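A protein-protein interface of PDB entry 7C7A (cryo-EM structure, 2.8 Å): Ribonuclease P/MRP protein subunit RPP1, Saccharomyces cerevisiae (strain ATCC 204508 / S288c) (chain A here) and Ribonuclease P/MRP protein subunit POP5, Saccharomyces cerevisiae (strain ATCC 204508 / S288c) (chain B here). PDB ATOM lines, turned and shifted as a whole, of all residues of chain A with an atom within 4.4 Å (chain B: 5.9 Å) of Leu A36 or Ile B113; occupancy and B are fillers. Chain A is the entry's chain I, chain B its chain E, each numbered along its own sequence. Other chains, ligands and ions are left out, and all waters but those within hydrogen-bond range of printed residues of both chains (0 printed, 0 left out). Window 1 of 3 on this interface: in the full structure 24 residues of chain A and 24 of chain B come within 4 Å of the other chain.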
ATOM      1  N   THR A  32      19.446   4.219  19.846  1.00  0.00           N
ATOM      2  CA  THR A  32      19.556   5.395  20.704  1.00  0.00           C
ATOM      3  C   THR A  32      20.689   6.305  20.243  1.00  0.00           C
ATOM      4  O   THR A  32      20.546   7.536  20.246  1.00  0.00           O
ATOM      5  CB  THR A  32      19.764   4.967  22.157  1.00  0.00           C
ATOM      6  OG1 THR A  32      18.645   4.185  22.587  1.00  0.00           O
ATOM      7  CG2 THR A  32      19.892   6.185  23.060  1.00  0.00           C
ATOM      8  N   LEU A  33      21.822   5.716  19.850  1.00  0.00           N
ATOM      9  CA  LEU A  33      22.928   6.496  19.301  1.00  0.00           C
ATOM     10  C   LEU A  33      22.486   7.299  18.086  1.00  0.00           C
ATOM     11  O   LEU A  33      22.751   8.504  17.998  1.00  0.00           O
ATOM     12  CB  LEU A  33      24.093   5.574  18.937  1.00  0.00           C
ATOM     13  CG  LEU A  33      25.288   5.525  19.891  1.00  0.00           C
ATOM     14  CD1 LEU A  33      24.875   4.973  21.239  1.00  0.00           C
ATOM     15  CD2 LEU A  33      26.409   4.689  19.294  1.00  0.00           C
ATOM     16  N   HIS A  34      21.808   6.648  17.138  1.00  0.00           N
ATOM     17  CA  HIS A  34      21.319   7.357  15.959  1.00  0.00           C
ATOM     18  C   HIS A  34      20.244   8.380  16.306  1.00  0.00           C
ATOM     19  O   HIS A  34      20.118   9.390  15.603  1.00  0.00           O
ATOM     20  CB  HIS A  34      20.780   6.366  14.928  1.00  0.00           C
ATOM     21  CG  HIS A  34      20.333   7.009  13.652  1.00  0.00           C
ATOM     22  ND1 HIS A  34      19.054   7.488  13.470  1.00  0.00           N
ATOM     23  CD2 HIS A  34      20.996   7.257  12.498  1.00  0.00           C
ATOM     24  CE1 HIS A  34      18.946   8.002  12.258  1.00  0.00           C
ATOM     25  NE2 HIS A  34      20.110   7.873  11.647  1.00  0.00           N
ATOM     26  N   MET A  35      19.471   8.142  17.367  1.00  0.00           N
ATOM     27  CA  MET A  35      18.456   9.103  17.783  1.00  0.00           C
ATOM     28  C   MET A  35      19.091  10.371  18.336  1.00  0.00           C
ATOM     29  O   MET A  35      18.663  11.484  18.004  1.00  0.00           O
ATOM     30  CB  MET A  35      17.536   8.467  18.825  1.00  0.00           C
ATOM     31  CG  MET A  35      16.420   9.375  19.305  1.00  0.00           C
ATOM     32  SD  MET A  35      15.211   9.706  18.011  1.00  0.00           S
ATOM     33  CE  MET A  35      14.530  11.260  18.578  1.00  0.00           C
ATOM     34  N   LEU A  36      20.114  10.227  19.182  1.00  0.00           N
ATOM     35  CA  LEU A  36      20.782  11.400  19.738  1.00  0.00           C
ATOM     36  C   LEU A  36      21.528  12.184  18.667  1.00  0.00           C
ATOM     37  O   LEU A  36      21.784  13.381  18.840  1.00  0.00           O
ATOM     38  CB  LEU A  36      21.737  10.982  20.856  1.00  0.00           C
ATOM     39  CG  LEU A  36      21.090  10.722  22.218  1.00  0.00           C
ATOM     40  CD1 LEU A  36      22.137  10.328  23.248  1.00  0.00           C
ATOM     41  CD2 LEU A  36      20.307  11.941  22.681  1.00  0.00           C
ATOM     42  N   GLY A  37      21.883  11.533  17.561  1.00  0.00           N
ATOM     43  CA  GLY A  37      22.546  12.199  16.459  1.00  0.00           C
ATOM     44  C   GLY A  37      23.988  11.773  16.282  1.00  0.00           C
ATOM     45  O   GLY A  37      24.882  12.272  16.971  1.00  0.00           O
ATOM     46  N   PRO A 198      21.330   1.363  26.408  1.00  0.00           N
ATOM     47  CA  PRO A 198      20.908   2.678  25.900  1.00  0.00           C
ATOM     48  C   PRO A 198      20.702   3.732  26.978  1.00  0.00           C
ATOM     49  O   PRO A 198      20.425   4.888  26.637  1.00  0.00           O
ATOM     50  CB  PRO A 198      19.588   2.362  25.178  1.00  0.00           C
ATOM     51  CG  PRO A 198      19.091   1.119  25.834  1.00  0.00           C
ATOM     52  CD  PRO A 198      20.313   0.324  26.174  1.00  0.00           C
ATOM     53  N   LEU A 199      20.830   3.385  28.258  1.00  0.00           N
ATOM     54  CA  LEU A 199      20.639   4.346  29.337  1.00  0.00           C
ATOM     55  C   LEU A 199      21.911   5.099  29.702  1.00  0.00           C
ATOM     56  O   LEU A 199      21.883   5.914  30.631  1.00  0.00           O
ATOM     57  CB  LEU A 199      20.090   3.640  30.581  1.00  0.00           C
ATOM     58  CG  LEU A 199      18.847   2.774  30.374  1.00  0.00           C
ATOM     59  CD1 LEU A 199      18.381   2.183  31.695  1.00  0.00           C
ATOM     60  CD2 LEU A 199      17.738   3.584  29.724  1.00  0.00           C
ATOM     61  N   CYS A 201      23.899   6.809  27.234  1.00  0.00           N
ATOM     62  CA  CYS A 201      24.233   7.465  25.976  1.00  0.00           C
ATOM     63  C   CYS A 201      24.001   8.964  26.111  1.00  0.00           C
ATOM     64  O   CYS A 201      22.988   9.389  26.676  1.00  0.00           O
ATOM     65  CB  CYS A 201      23.393   6.896  24.833  1.00  0.00           C
ATOM     66  SG  CYS A 201      23.668   5.136  24.532  1.00  0.00           S
ATOM     67  N   ARG A 202      24.937   9.758  25.597  1.00  0.00           N
ATOM     68  CA  ARG A 202      24.880  11.208  25.700  1.00  0.00           C
ATOM     69  C   ARG A 202      25.136  11.845  24.340  1.00  0.00           C
ATOM     70  O   ARG A 202      25.423  11.169  23.349  1.00  0.00           O
ATOM     71  CB  ARG A 202      25.890  11.723  26.734  1.00  0.00           C
ATOM     72  CG  ARG A 202      25.620  11.229  28.146  1.00  0.00           C
ATOM     73  CD  ARG A 202      24.257  11.694  28.629  1.00  0.00           C
ATOM     74  NE  ARG A 202      24.025  11.364  30.032  1.00  0.00           N
ATOM     75  CZ  ARG A 202      23.468  10.233  30.452  1.00  0.00           C
ATOM     76  NH1 ARG A 202      23.295  10.020  31.749  1.00  0.00           N
ATOM     77  NH2 ARG A 202      23.086   9.314  29.576  1.00  0.00           N
ATOM     78  N   ASN A 203      25.029  13.171  24.303  1.00  0.00           N
ATOM     79  CA  ASN A 203      25.139  13.956  23.082  1.00  0.00           C
ATOM     80  C   ASN A 203      26.516  14.610  22.999  1.00  0.00           C
ATOM     81  O   ASN A 203      27.389  14.400  23.846  1.00  0.00           O
ATOM     82  CB  ASN A 203      24.026  15.004  23.019  1.00  0.00           C
ATOM     83  CG  ASN A 203      23.661  15.386  21.596  1.00  0.00           C
ATOM     84  OD1 ASN A 203      24.104  14.753  20.638  1.00  0.00           O
ATOM     85  ND2 ASN A 203      22.848  16.426  21.452  1.00  0.00           N
ATOM     86  N   GLU B  12      16.144  18.315  26.396  1.00  0.00           N
ATOM     87  CA  GLU B  12      15.065  17.391  26.078  1.00  0.00           C
ATOM     88  C   GLU B  12      15.217  16.129  26.911  1.00  0.00           C
ATOM     89  O   GLU B  12      16.335  15.657  27.141  1.00  0.00           O
ATOM     90  CB  GLU B  12      15.067  17.040  24.583  1.00  0.00           C
ATOM     91  CG  GLU B  12      13.952  16.103  24.145  1.00  0.00           C
ATOM     92  CD  GLU B  12      12.577  16.732  24.246  1.00  0.00           C
ATOM     93  OE1 GLU B  12      12.474  17.972  24.153  1.00  0.00           O
ATOM     94  OE2 GLU B  12      11.594  15.981  24.417  1.00  0.00           O
ATOM     95  N   ILE B  13      14.093  15.586  27.365  1.00  0.00           N
ATOM     96  CA  ILE B  13      14.080  14.333  28.112  1.00  0.00           C
ATOM     97  C   ILE B  13      13.687  13.215  27.156  1.00  0.00           C
ATOM     98  O   ILE B  13      12.557  13.182  26.657  1.00  0.00           O
ATOM     99  CB  ILE B  13      13.116  14.405  29.305  1.00  0.00           C
ATOM    100  CG1 ILE B  13      13.571  15.479  30.296  1.00  0.00           C
ATOM    101  CG2 ILE B  13      13.010  13.050  29.985  1.00  0.00           C
ATOM    102  CD1 ILE B  13      12.703  15.577  31.533  1.00  0.00           C
ATOM    103  N   ILE B  14      14.617  12.297  26.899  1.00  0.00           N
ATOM    104  CA  ILE B  14      14.414  11.211  25.947  1.00  0.00           C
ATOM    105  C   ILE B  14      14.392   9.897  26.715  1.00  0.00           C
ATOM    106  O   ILE B  14      15.263   9.648  27.555  1.00  0.00           O
ATOM    107  CB  ILE B  14      15.505  11.197  24.862  1.00  0.00           C
ATOM    108  CG1 ILE B  14      15.525  12.530  24.111  1.00  0.00           C
ATOM    109  CG2 ILE B  14      15.287  10.043  23.896  1.00  0.00           C
ATOM    110  CD1 ILE B  14      16.556  12.595  23.006  1.00  0.00           C
ATOM    111  N   PHE B  15      13.395   9.060  26.427  1.00  0.00           N
ATOM    112  CA  PHE B  15      13.254   7.778  27.100  1.00  0.00           C
ATOM    113  C   PHE B  15      13.679   6.663  26.160  1.00  0.00           C
ATOM    114  O   PHE B  15      12.962   6.379  25.188  1.00  0.00           O
ATOM    115  CB  PHE B  15      11.812   7.567  27.558  1.00  0.00           C
ATOM    116  CG  PHE B  15      11.406   8.442  28.707  1.00  0.00           C
ATOM    117  CD1 PHE B  15      11.606   8.028  30.013  1.00  0.00           C
ATOM    118  CD2 PHE B  15      10.825   9.680  28.483  1.00  0.00           C
ATOM    119  CE1 PHE B  15      11.235   8.829  31.074  1.00  0.00           C
ATOM    120  CE2 PHE B  15      10.451  10.486  29.541  1.00  0.00           C
ATOM    121  CZ  PHE B  15      10.657  10.061  30.838  1.00  0.00           C
ATOM    122  N   PRO B  16      14.821   6.011  26.389  1.00  0.00           N
ATOM    123  CA  PRO B  16      15.210   4.902  25.523  1.00  0.00           C
ATOM    124  C   PRO B  16      14.305   3.706  25.747  1.00  0.00           C
ATOM    125  O   PRO B  16      14.033   3.321  26.899  1.00  0.00           O
ATOM    126  CB  PRO B  16      16.657   4.601  25.958  1.00  0.00           C
ATOM    127  CG  PRO B  16      17.096   5.804  26.742  1.00  0.00           C
ATOM    128  CD  PRO B  16      15.856   6.324  27.387  1.00  0.00           C
ATOM    129  N   MET B 103      23.177  13.723  34.470  1.00  0.00           N
ATOM    130  CA  MET B 103      21.911  13.438  35.140  1.00  0.00           C
ATOM    131  C   MET B 103      21.628  11.944  35.052  1.00  0.00           C
ATOM    132  O   MET B 103      21.512  11.389  33.955  1.00  0.00           O
ATOM    133  CB  MET B 103      20.781  14.248  34.512  1.00  0.00           C
ATOM    134  CG  MET B 103      19.469  14.169  35.278  1.00  0.00           C
ATOM    135  SD  MET B 103      18.378  15.567  34.956  1.00  0.00           S
ATOM    136  CE  MET B 103      19.244  16.883  35.808  1.00  0.00           C
ATOM    137  N   GLY B 111      15.368   5.283  33.977  1.00  0.00           N
ATOM    138  CA  GLY B 111      15.474   4.971  32.566  1.00  0.00           C
ATOM    139  C   GLY B 111      15.181   6.144  31.655  1.00  0.00           C
ATOM    140  O   GLY B 111      14.219   6.112  30.881  1.00  0.00           O
ATOM    141  N   LEU B 112      16.008   7.184  31.731  1.00  0.00           N
ATOM    142  CA  LEU B 112      15.811   8.376  30.918  1.00  0.00           C
ATOM    143  C   LEU B 112      17.146   9.082  30.742  1.00  0.00           C
ATOM    144  O   LEU B 112      18.044   8.961  31.581  1.00  0.00           O
ATOM    145  CB  LEU B 112      14.783   9.328  31.543  1.00  0.00           C
ATOM    146  CG  LEU B 112      15.209  10.143  32.768  1.00  0.00           C
ATOM    147  CD1 LEU B 112      14.266  11.316  32.972  1.00  0.00           C
ATOM    148  CD2 LEU B 112      15.258   9.284  34.024  1.00  0.00           C
ATOM    149  N   ILE B 113      17.265   9.821  29.639  1.00  0.00           N
ATOM    150  CA  ILE B 113      18.467  10.580  29.329  1.00  0.00           C
ATOM    151  C   ILE B 113      18.080  12.026  29.042  1.00  0.00           C
ATOM    152  O   ILE B 113      16.944  12.335  28.665  1.00  0.00           O
ATOM    153  CB  ILE B 113      19.250   9.981  28.141  1.00  0.00           C
ATOM    154  CG1 ILE B 113      18.410  10.027  26.864  1.00  0.00           C
ATOM    155  CG2 ILE B 113      19.686   8.555  28.449  1.00  0.00           C
ATOM    156  CD1 ILE B 113      19.125   9.491  25.642  1.00  0.00           C
ATOM    157  N   VAL B 114      19.052  12.917  29.226  1.00  0.00           N
ATOM    158  CA  VAL B 114      18.880  14.347  29.001  1.00  0.00           C
ATOM    159  C   VAL B 114      19.784  14.760  27.849  1.00  0.00           C
ATOM    160  O   VAL B 114      20.987  14.469  27.860  1.00  0.00           O
ATOM    161  CB  VAL B 114      19.198  15.164  30.267  1.00  0.00           C
ATOM    162  CG1 VAL B 114      18.999  16.649  30.005  1.00  0.00           C
ATOM    163  CG2 VAL B 114      18.330  14.700  31.426  1.00  0.00           C
ATOM    164  N   ASN B 115      19.205  15.436  26.861  1.00  0.00           N
ATOM    165  CA  ASN B 115      19.931  15.856  25.669  1.00  0.00           C
ATOM    166  C   ASN B 115      19.898  17.373  25.555  1.00  0.00           C
ATOM    167  O   ASN B 115      18.818  17.947  25.347  1.00  0.00           O
ATOM    168  CB  ASN B 115      19.322  15.211  24.422  1.00  0.00           C
ATOM    169  CG  ASN B 115      19.936  15.726  23.133  1.00  0.00           C
ATOM    170  OD1 ASN B 115      21.075  16.191  23.112  1.00  0.00           O
ATOM    171  ND2 ASN B 115      19.178  15.644  22.046  1.00  0.00           N
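The backbone carbonyl oxygen (O) of Met B103 lies within hydrogen-bond range of the guanidinium group (NH1) of Arg A202 (3.1 Å). ND2 of Asn A203 lies within hydrogen-bond range of OD1 of Asn B115 (2.4 Å).
The backbone carbonyl oxygen (O) of Glu B12 sits at hydrogen-bond distance from the backbone NH (N) of Asn B115 (2.9 Å). N of Ile B113 lies within hydrogen-bond range of O of Ile B14 (2.9 Å). O of Leu A36 sits close to OD1 of Asn A203 (3.2 Å).
OG1 of Thr A32 touches CB of Pro B16 (3.9 Å). Leu A36 touches Ile B14. CD1 of Leu A36 touches CD1 of Ile B113 (3.9 Å). CD2 of Leu A36 touches CG of Asn B115 (3.8 Å). Pro A198 touches Pro B16 (O to CG, 3.5 Å). CD2 of Leu A199 touches CG of Pro B16 (3.8 Å). Gly B111 touches Leu A199. Cys A201 touches Ile B113 (O to CG2, 3.8 Å). Ile B113 touches Arg A202 (CG2 to NH2, 3.7 Å).
Of chain B, only Ile B14, Ile B113 and Asn B115 come within 4 Å of Leu A36. Of chain A, only Leu A36 (3.9 Å), Cys A201 (3.8 Å) and Arg A202 (3.7 Å) come within 4 Å of Ile B113. Of the printed residues of chain B, Asn A203 touches Asn B115. Of the printed residues of chain A, Ile B14 touches Leu A36. Of the printed residues of chain B, Thr A32 touches Pro B16. Of the printed residues of chain A, Asn B115 touches Leu A36 (3.8 Å) and Asn A203 (2.4 Å). Of the printed residues of chain A, Gly B111 touches Leu A199 (3.9 Å). The nearest residue of chain B that does not touch Leu A36 is Val B114 (5.8 Å). The nearest residue of chain A that does not touch Ile B113 is Leu A199 (4.1 Å). The nearest printed residue of chain B that does not touch Thr A32 is Ile B113 (4.3 Å).
Printed residues of chain A that touch a printed residue of chain B: Thr A32, Leu A36, Pro A198, Leu A199, Cys A201, Arg A202 and Asn A203. Hydrophobic or aromatic side chains of chain A that line the printed part of chain B: Leu A36, Pro A198 and Leu A199. Along chain A the printed residues that touch a printed residue of chain B span positions 32 to 203. Among the printed residues, 11 pairs touch across the chains.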
